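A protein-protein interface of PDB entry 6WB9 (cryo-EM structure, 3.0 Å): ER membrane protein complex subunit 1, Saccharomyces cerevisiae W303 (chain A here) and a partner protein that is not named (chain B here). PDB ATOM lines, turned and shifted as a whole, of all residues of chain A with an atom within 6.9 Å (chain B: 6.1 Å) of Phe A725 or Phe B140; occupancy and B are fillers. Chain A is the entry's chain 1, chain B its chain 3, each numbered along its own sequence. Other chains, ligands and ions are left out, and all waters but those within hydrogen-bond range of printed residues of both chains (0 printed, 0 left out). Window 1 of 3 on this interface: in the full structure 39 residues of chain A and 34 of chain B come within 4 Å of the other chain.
OG of Ser B176 is in hydrogen-bond range of O of Phe B140 (3.2 Å).
Among the printed residues, merely in contact across the chains: Phe A725 with Phe B139 (3.3 Å), Leu A730 with Phe B140 (3.4 Å), Leu A730 with Trp B10 (3.4 Å), Met A721 with Trp B10 (3.5 Å), Leu A730 with Pro B14 (3.6 Å), Lys A727 with Trp B10 (3.6 Å), Glu A726 with Phe B139 (3.6 Å), Lys A729 with Phe B139 (3.6 Å), Met A721 with Leu B7 (3.6 Å), Phe A725 with Phe B140 (3.7 Å), Leu A730 with Phe B139 (3.8 Å), Phe A725 with Phe B143 (3.8 Å) and Leu A730 with Trp B135 (3.9 Å).
Thr A724 touches none of the printed residues of chain B. Phe A725 touches just these residues of chain B: Phe B139 (3.3 Å), Phe B140 (3.7 Å) and Phe B143 (3.8 Å). Of the printed residues of chain A, Trp B10 touches Met A721, Lys A727 and Leu A730. His B138 touches none of the printed residues of chain A. Printed residues of chain A within 4 Å of Phe B139: Phe A725 (3.3 Å), Glu A726 (3.6 Å), Lys A729 (3.6 Å) and Leu A730 (3.8 Å). Phe B140 touches just these residues of chain A: Phe A725 and Leu A730. The nearest printed residue of chain A that does not touch Trp B135 is Lys A729 (5.6 Å).
Of the 17 printed residues of chain B, 7 touch a printed residue of chain A. Hydrophobic or aromatic side chains of chain B within 4 Å of the printed part of chain A: Leu B7, Trp B10, Pro B14, Trp B135, Phe B139, Phe B140 and Phe B143. Among the printed residues, 13 pairs touch across the chains. Among the printed residues, no Asp or Glu carboxylate lies within 4 Å of a Lys or Arg side-chain nitrogen of the other chain.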
ATOM      1  N   MET A 721     -36.000 -12.837 -19.322  1.00  0.00           N
ATOM      2  CA  MET A 721     -35.234 -13.334 -20.458  1.00  0.00           C
ATOM      3  C   MET A 721     -35.894 -12.864 -21.748  1.00  0.00           C
ATOM      4  O   MET A 721     -37.112 -12.964 -21.900  1.00  0.00           O
ATOM      5  CB  MET A 721     -35.164 -14.857 -20.424  1.00  0.00           C
ATOM      6  CG  MET A 721     -34.323 -15.462 -21.533  1.00  0.00           C
ATOM      7  SD  MET A 721     -34.184 -17.250 -21.374  1.00  0.00           S
ATOM      8  CE  MET A 721     -32.953 -17.376 -20.079  1.00  0.00           C
ATOM      9  N   SER A 722     -35.087 -12.378 -22.684  1.00  0.00           N
ATOM     10  CA  SER A 722     -35.606 -11.839 -23.928  1.00  0.00           C
ATOM     11  C   SER A 722     -36.270 -12.940 -24.757  1.00  0.00           C
ATOM     12  O   SER A 722     -35.879 -14.108 -24.674  1.00  0.00           O
ATOM     13  CB  SER A 722     -34.481 -11.190 -24.731  1.00  0.00           C
ATOM     14  OG  SER A 722     -34.940 -10.710 -25.982  1.00  0.00           O
ATOM     15  N   PRO A 723     -37.309 -12.597 -25.530  1.00  0.00           N
ATOM     16  CA  PRO A 723     -37.901 -13.598 -26.435  1.00  0.00           C
ATOM     17  C   PRO A 723     -36.952 -14.047 -27.531  1.00  0.00           C
ATOM     18  O   PRO A 723     -36.955 -15.228 -27.901  1.00  0.00           O
ATOM     19  CB  PRO A 723     -39.126 -12.869 -27.003  1.00  0.00           C
ATOM     20  CG  PRO A 723     -39.454 -11.834 -25.984  1.00  0.00           C
ATOM     21  CD  PRO A 723     -38.136 -11.382 -25.439  1.00  0.00           C
ATOM     22  N   THR A 724     -36.139 -13.140 -28.062  1.00  0.00           N
ATOM     23  CA  THR A 724     -35.087 -13.510 -29.005  1.00  0.00           C
ATOM     24  C   THR A 724     -33.751 -13.660 -28.278  1.00  0.00           C
ATOM     25  O   THR A 724     -32.755 -13.012 -28.602  1.00  0.00           O
ATOM     26  CB  THR A 724     -34.992 -12.485 -30.129  1.00  0.00           C
ATOM     27  OG1 THR A 724     -34.406 -11.278 -29.627  1.00  0.00           O
ATOM     28  CG2 THR A 724     -36.376 -12.184 -30.686  1.00  0.00           C
ATOM     29  N   PHE A 725     -33.747 -14.527 -27.269  1.00  0.00           N
ATOM     30  CA  PHE A 725     -32.520 -14.920 -26.593  1.00  0.00           C
ATOM     31  C   PHE A 725     -31.929 -16.118 -27.321  1.00  0.00           C
ATOM     32  O   PHE A 725     -32.622 -17.114 -27.556  1.00  0.00           O
ATOM     33  CB  PHE A 725     -32.777 -15.257 -25.124  1.00  0.00           C
ATOM     34  CG  PHE A 725     -31.545 -15.674 -24.374  1.00  0.00           C
ATOM     35  CD1 PHE A 725     -30.558 -14.752 -24.067  1.00  0.00           C
ATOM     36  CD2 PHE A 725     -31.374 -16.988 -23.975  1.00  0.00           C
ATOM     37  CE1 PHE A 725     -29.423 -15.137 -23.378  1.00  0.00           C
ATOM     38  CE2 PHE A 725     -30.242 -17.380 -23.286  1.00  0.00           C
ATOM     39  CZ  PHE A 725     -29.266 -16.453 -22.987  1.00  0.00           C
ATOM     40  N   GLU A 726     -30.652 -16.017 -27.682  1.00  0.00           N
ATOM     41  CA  GLU A 726     -30.005 -17.000 -28.549  1.00  0.00           C
ATOM     42  C   GLU A 726     -29.684 -18.258 -27.747  1.00  0.00           C
ATOM     43  O   GLU A 726     -28.546 -18.509 -27.345  1.00  0.00           O
ATOM     44  CB  GLU A 726     -28.755 -16.402 -29.180  1.00  0.00           C
ATOM     45  CG  GLU A 726     -29.016 -15.134 -29.979  1.00  0.00           C
ATOM     46  CD  GLU A 726     -27.741 -14.396 -30.341  1.00  0.00           C
ATOM     47  OE1 GLU A 726     -26.673 -14.752 -29.803  1.00  0.00           O
ATOM     48  OE2 GLU A 726     -27.808 -13.458 -31.163  1.00  0.00           O
ATOM     49  N   LYS A 727     -30.722 -19.069 -27.511  1.00  0.00           N
ATOM     50  CA  LYS A 727     -30.519 -20.373 -26.887  1.00  0.00           C
ATOM     51  C   LYS A 727     -29.902 -21.368 -27.858  1.00  0.00           C
ATOM     52  O   LYS A 727     -29.152 -22.260 -27.441  1.00  0.00           O
ATOM     53  CB  LYS A 727     -31.844 -20.927 -26.365  1.00  0.00           C
ATOM     54  CG  LYS A 727     -32.378 -20.253 -25.122  1.00  0.00           C
ATOM     55  CD  LYS A 727     -33.648 -20.937 -24.649  1.00  0.00           C
ATOM     56  CE  LYS A 727     -34.133 -20.363 -23.332  1.00  0.00           C
ATOM     57  NZ  LYS A 727     -35.370 -21.042 -22.856  1.00  0.00           N
ATOM     58  N   GLY A 728     -30.214 -21.232 -29.149  1.00  0.00           N
ATOM     59  CA  GLY A 728     -29.691 -22.163 -30.136  1.00  0.00           C
ATOM     60  C   GLY A 728     -28.194 -22.022 -30.330  1.00  0.00           C
ATOM     61  O   GLY A 728     -27.465 -23.015 -30.337  1.00  0.00           O
ATOM     62  N   LYS A 729     -27.714 -20.781 -30.459  1.00  0.00           N
ATOM     63  CA  LYS A 729     -26.277 -20.548 -30.558  1.00  0.00           C
ATOM     64  C   LYS A 729     -25.568 -20.866 -29.247  1.00  0.00           C
ATOM     65  O   LYS A 729     -24.397 -21.262 -29.259  1.00  0.00           O
ATOM     66  CB  LYS A 729     -26.008 -19.103 -30.971  1.00  0.00           C
ATOM     67  CG  LYS A 729     -26.804 -18.639 -32.176  1.00  0.00           C
ATOM     68  CD  LYS A 729     -26.613 -17.150 -32.421  1.00  0.00           C
ATOM     69  CE  LYS A 729     -27.462 -16.671 -33.586  1.00  0.00           C
ATOM     70  NZ  LYS A 729     -28.911 -16.918 -33.357  1.00  0.00           N
ATOM     71  N   LEU A 730     -26.276 -20.737 -28.122  1.00  0.00           N
ATOM     72  CA  LEU A 730     -25.735 -21.118 -26.820  1.00  0.00           C
ATOM     73  C   LEU A 730     -25.465 -22.619 -26.758  1.00  0.00           C
ATOM     74  O   LEU A 730     -24.353 -23.053 -26.420  1.00  0.00           O
ATOM     75  CB  LEU A 730     -26.719 -20.686 -25.729  1.00  0.00           C
ATOM     76  CG  LEU A 730     -26.539 -20.968 -24.239  1.00  0.00           C
ATOM     77  CD1 LEU A 730     -25.295 -20.276 -23.709  1.00  0.00           C
ATOM     78  CD2 LEU A 730     -27.771 -20.556 -23.463  1.00  0.00           C
ATOM     79  N   LEU B   7     -33.317 -17.192 -16.464  1.00  0.00           N
ATOM     80  CA  LEU B   7     -32.045 -16.475 -16.514  1.00  0.00           C
ATOM     81  C   LEU B   7     -30.974 -17.202 -15.716  1.00  0.00           C
ATOM     82  O   LEU B   7     -29.840 -17.345 -16.183  1.00  0.00           O
ATOM     83  CB  LEU B   7     -32.214 -15.050 -15.990  1.00  0.00           C
ATOM     84  CG  LEU B   7     -32.870 -14.034 -16.920  1.00  0.00           C
ATOM     85  CD1 LEU B   7     -32.864 -12.664 -16.275  1.00  0.00           C
ATOM     86  CD2 LEU B   7     -32.153 -14.004 -18.253  1.00  0.00           C
ATOM     87  N   TRP B  10     -30.177 -20.617 -17.541  1.00  0.00           N
ATOM     88  CA  TRP B  10     -29.593 -20.478 -18.865  1.00  0.00           C
ATOM     89  C   TRP B  10     -28.422 -19.510 -18.927  1.00  0.00           C
ATOM     90  O   TRP B  10     -27.888 -19.287 -20.018  1.00  0.00           O
ATOM     91  CB  TRP B  10     -30.663 -20.039 -19.873  1.00  0.00           C
ATOM     92  CG  TRP B  10     -31.617 -21.128 -20.232  1.00  0.00           C
ATOM     93  CD1 TRP B  10     -32.760 -21.471 -19.570  1.00  0.00           C
ATOM     94  CD2 TRP B  10     -31.510 -22.027 -21.342  1.00  0.00           C
ATOM     95  NE1 TRP B  10     -33.372 -22.527 -20.201  1.00  0.00           N
ATOM     96  CE2 TRP B  10     -32.625 -22.886 -21.291  1.00  0.00           C
ATOM     97  CE3 TRP B  10     -30.580 -22.186 -22.373  1.00  0.00           C
ATOM     98  CZ2 TRP B  10     -32.836 -23.891 -22.233  1.00  0.00           C
ATOM     99  CZ3 TRP B  10     -30.790 -23.182 -23.306  1.00  0.00           C
ATOM    100  CH2 TRP B  10     -31.909 -24.023 -23.230  1.00  0.00           C
ATOM    101  N   VAL B  11     -28.007 -18.919 -17.804  1.00  0.00           N
ATOM    102  CA  VAL B  11     -26.809 -18.100 -17.758  1.00  0.00           C
ATOM    103  C   VAL B  11     -25.772 -18.656 -16.787  1.00  0.00           C
ATOM    104  O   VAL B  11     -24.584 -18.705 -17.117  1.00  0.00           O
ATOM    105  CB  VAL B  11     -27.156 -16.628 -17.424  1.00  0.00           C
ATOM    106  CG1 VAL B  11     -25.915 -15.782 -17.268  1.00  0.00           C
ATOM    107  CG2 VAL B  11     -28.023 -16.031 -18.515  1.00  0.00           C
ATOM    108  N   PRO B  14     -24.604 -22.418 -18.257  1.00  0.00           N
ATOM    109  CA  PRO B  14     -23.833 -22.354 -19.514  1.00  0.00           C
ATOM    110  C   PRO B  14     -22.513 -21.609 -19.418  1.00  0.00           C
ATOM    111  O   PRO B  14     -21.545 -22.035 -20.057  1.00  0.00           O
ATOM    112  CB  PRO B  14     -24.801 -21.658 -20.473  1.00  0.00           C
ATOM    113  CG  PRO B  14     -26.101 -22.074 -20.007  1.00  0.00           C
ATOM    114  CD  PRO B  14     -25.999 -22.005 -18.528  1.00  0.00           C
ATOM    115  N   ILE B  15     -22.437 -20.518 -18.650  1.00  0.00           N
ATOM    116  CA  ILE B  15     -21.169 -19.805 -18.499  1.00  0.00           C
ATOM    117  C   ILE B  15     -20.162 -20.664 -17.740  1.00  0.00           C
ATOM    118  O   ILE B  15     -18.982 -20.726 -18.106  1.00  0.00           O
ATOM    119  CB  ILE B  15     -21.399 -18.439 -17.821  1.00  0.00           C
ATOM    120  CG1 ILE B  15     -22.079 -17.474 -18.788  1.00  0.00           C
ATOM    121  CG2 ILE B  15     -20.105 -17.811 -17.350  1.00  0.00           C
ATOM    122  CD1 ILE B  15     -22.319 -16.101 -18.210  1.00  0.00           C
ATOM    123  N   TRP B 135     -17.642 -13.169 -25.104  1.00  0.00           N
ATOM    124  CA  TRP B 135     -18.782 -14.044 -25.350  1.00  0.00           C
ATOM    125  C   TRP B 135     -19.851 -13.895 -24.274  1.00  0.00           C
ATOM    126  O   TRP B 135     -21.047 -13.973 -24.577  1.00  0.00           O
ATOM    127  CB  TRP B 135     -18.303 -15.490 -25.444  1.00  0.00           C
ATOM    128  CG  TRP B 135     -19.390 -16.487 -25.600  1.00  0.00           C
ATOM    129  CD1 TRP B 135     -20.040 -16.816 -26.750  1.00  0.00           C
ATOM    130  CD2 TRP B 135     -19.950 -17.309 -24.573  1.00  0.00           C
ATOM    131  NE1 TRP B 135     -20.979 -17.786 -26.502  1.00  0.00           N
ATOM    132  CE2 TRP B 135     -20.942 -18.106 -25.171  1.00  0.00           C
ATOM    133  CE3 TRP B 135     -19.711 -17.444 -23.202  1.00  0.00           C
ATOM    134  CZ2 TRP B 135     -21.694 -19.024 -24.448  1.00  0.00           C
ATOM    135  CZ3 TRP B 135     -20.458 -18.353 -22.488  1.00  0.00           C
ATOM    136  CH2 TRP B 135     -21.438 -19.131 -23.111  1.00  0.00           C
ATOM    137  N   VAL B 136     -19.439 -13.658 -23.027  1.00  0.00           N
ATOM    138  CA  VAL B 136     -20.396 -13.371 -21.961  1.00  0.00           C
ATOM    139  C   VAL B 136     -21.046 -12.008 -22.184  1.00  0.00           C
ATOM    140  O   VAL B 136     -22.270 -11.863 -22.089  1.00  0.00           O
ATOM    141  CB  VAL B 136     -19.708 -13.463 -20.586  1.00  0.00           C
ATOM    142  CG1 VAL B 136     -20.593 -12.904 -19.495  1.00  0.00           C
ATOM    143  CG2 VAL B 136     -19.365 -14.902 -20.269  1.00  0.00           C
ATOM    144  N   ASN B 137     -20.244 -10.996 -22.533  1.00  0.00           N
ATOM    145  CA  ASN B 137     -20.792  -9.664 -22.779  1.00  0.00           C
ATOM    146  C   ASN B 137     -21.531  -9.545 -24.109  1.00  0.00           C
ATOM    147  O   ASN B 137     -22.110  -8.490 -24.379  1.00  0.00           O
ATOM    148  CB  ASN B 137     -19.677  -8.620 -22.719  1.00  0.00           C
ATOM    149  CG  ASN B 137     -19.340  -8.210 -21.302  1.00  0.00           C
ATOM    150  OD1 ASN B 137     -20.207  -8.184 -20.431  1.00  0.00           O
ATOM    151  ND2 ASN B 137     -18.077  -7.881 -21.065  1.00  0.00           N
ATOM    152  N   HIS B 138     -21.500 -10.570 -24.955  1.00  0.00           N
ATOM    153  CA  HIS B 138     -22.268 -10.587 -26.193  1.00  0.00           C
ATOM    154  C   HIS B 138     -23.537 -11.421 -26.094  1.00  0.00           C
ATOM    155  O   HIS B 138     -24.588 -10.998 -26.583  1.00  0.00           O
ATOM    156  CB  HIS B 138     -21.401 -11.114 -27.341  1.00  0.00           C
ATOM    157  CG  HIS B 138     -22.153 -11.349 -28.616  1.00  0.00           C
ATOM    158  ND1 HIS B 138     -22.867 -10.356 -29.253  1.00  0.00           N
ATOM    159  CD2 HIS B 138     -22.296 -12.461 -29.374  1.00  0.00           C
ATOM    160  CE1 HIS B 138     -23.421 -10.849 -30.347  1.00  0.00           C
ATOM    161  NE2 HIS B 138     -23.090 -12.124 -30.443  1.00  0.00           N
ATOM    162  N   PHE B 139     -23.468 -12.594 -25.471  1.00  0.00           N
ATOM    163  CA  PHE B 139     -24.631 -13.467 -25.380  1.00  0.00           C
ATOM    164  C   PHE B 139     -25.537 -13.142 -24.205  1.00  0.00           C
ATOM    165  O   PHE B 139     -26.741 -13.416 -24.271  1.00  0.00           O
ATOM    166  CB  PHE B 139     -24.185 -14.925 -25.269  1.00  0.00           C
ATOM    167  CG  PHE B 139     -24.027 -15.611 -26.586  1.00  0.00           C
ATOM    168  CD1 PHE B 139     -24.882 -16.639 -26.947  1.00  0.00           C
ATOM    169  CD2 PHE B 139     -23.031 -15.228 -27.468  1.00  0.00           C
ATOM    170  CE1 PHE B 139     -24.740 -17.277 -28.160  1.00  0.00           C
ATOM    171  CE2 PHE B 139     -22.885 -15.861 -28.688  1.00  0.00           C
ATOM    172  CZ  PHE B 139     -23.742 -16.887 -29.034  1.00  0.00           C
ATOM    173  N   PHE B 140     -24.996 -12.571 -23.127  1.00  0.00           N
ATOM    174  CA  PHE B 140     -25.745 -12.461 -21.883  1.00  0.00           C
ATOM    175  C   PHE B 140     -25.807 -11.036 -21.351  1.00  0.00           C
ATOM    176  O   PHE B 140     -26.133 -10.836 -20.177  1.00  0.00           O
ATOM    177  CB  PHE B 140     -25.153 -13.384 -20.819  1.00  0.00           C
ATOM    178  CG  PHE B 140     -24.927 -14.783 -21.291  1.00  0.00           C
ATOM    179  CD1 PHE B 140     -25.989 -15.655 -21.446  1.00  0.00           C
ATOM    180  CD2 PHE B 140     -23.652 -15.226 -21.578  1.00  0.00           C
ATOM    181  CE1 PHE B 140     -25.782 -16.943 -21.876  1.00  0.00           C
ATOM    182  CE2 PHE B 140     -23.440 -16.509 -22.011  1.00  0.00           C
ATOM    183  CZ  PHE B 140     -24.505 -17.369 -22.161  1.00  0.00           C
ATOM    184  N   ALA B 141     -25.501 -10.042 -22.174  1.00  0.00           N
ATOM    185  CA  ALA B 141     -25.621  -8.666 -21.727  1.00  0.00           C
ATOM    186  C   ALA B 141     -27.066  -8.205 -21.825  1.00  0.00           C
ATOM    187  O   ALA B 141     -27.828  -8.651 -22.686  1.00  0.00           O
ATOM    188  CB  ALA B 141     -24.728  -7.742 -22.551  1.00  0.00           C
ATOM    189  N   GLY B 142     -27.440  -7.306 -20.921  1.00  0.00           N
ATOM    190  CA  GLY B 142     -28.750  -6.696 -20.949  1.00  0.00           C
ATOM    191  C   GLY B 142     -29.683  -7.109 -19.837  1.00  0.00           C
ATOM    192  O   GLY B 142     -30.793  -6.569 -19.763  1.00  0.00           O
ATOM    193  N   PHE B 143     -29.292  -8.040 -18.971  1.00  0.00           N
ATOM    194  CA  PHE B 143     -30.159  -8.421 -17.869  1.00  0.00           C
ATOM    195  C   PHE B 143     -29.358  -8.666 -16.602  1.00  0.00           C
ATOM    196  O   PHE B 143     -28.200  -9.083 -16.643  1.00  0.00           O
ATOM    197  CB  PHE B 143     -31.010  -9.660 -18.186  1.00  0.00           C
ATOM    198  CG  PHE B 143     -30.302 -10.711 -18.976  1.00  0.00           C
ATOM    199  CD1 PHE B 143     -30.559 -10.858 -20.328  1.00  0.00           C
ATOM    200  CD2 PHE B 143     -29.403 -11.571 -18.369  1.00  0.00           C
ATOM    201  CE1 PHE B 143     -29.920 -11.833 -21.063  1.00  0.00           C
ATOM    202  CE2 PHE B 143     -28.761 -12.543 -19.098  1.00  0.00           C
ATOM    203  CZ  PHE B 143     -29.024 -12.677 -20.445  1.00  0.00           C
ATOM    204  N   THR B 162     -23.474  -4.111 -16.457  1.00  0.00           N
ATOM    205  CA  THR B 162     -22.988  -3.581 -17.725  1.00  0.00           C
ATOM    206  C   THR B 162     -24.100  -2.993 -18.585  1.00  0.00           C
ATOM    207  O   THR B 162     -24.025  -1.823 -18.970  1.00  0.00           O
ATOM    208  CB  THR B 162     -22.242  -4.674 -18.502  1.00  0.00           C
ATOM    209  OG1 THR B 162     -23.052  -5.854 -18.572  1.00  0.00           O
ATOM    210  CG2 THR B 162     -20.925  -5.001 -17.825  1.00  0.00           C
ATOM    211  N   SER B 175     -24.775  -8.450 -13.289  1.00  0.00           N
ATOM    212  CA  SER B 175     -24.926  -9.011 -14.623  1.00  0.00           C
ATOM    213  C   SER B 175     -24.134 -10.314 -14.724  1.00  0.00           C
ATOM    214  O   SER B 175     -23.682 -10.879 -13.725  1.00  0.00           O
ATOM    215  CB  SER B 175     -24.496  -7.996 -15.675  1.00  0.00           C
ATOM    216  OG  SER B 175     -23.145  -7.624 -15.490  1.00  0.00           O
ATOM    217  N   SER B 176     -23.960 -10.812 -15.948  1.00  0.00           N
ATOM    218  CA  SER B 176     -23.302 -12.094 -16.158  1.00  0.00           C
ATOM    219  C   SER B 176     -21.784 -11.990 -16.164  1.00  0.00           C
ATOM    220  O   SER B 176     -21.104 -12.994 -15.908  1.00  0.00           O
ATOM    221  CB  SER B 176     -23.780 -12.703 -17.470  1.00  0.00           C
ATOM    222  OG  SER B 176     -25.175 -12.521 -17.616  1.00  0.00           O
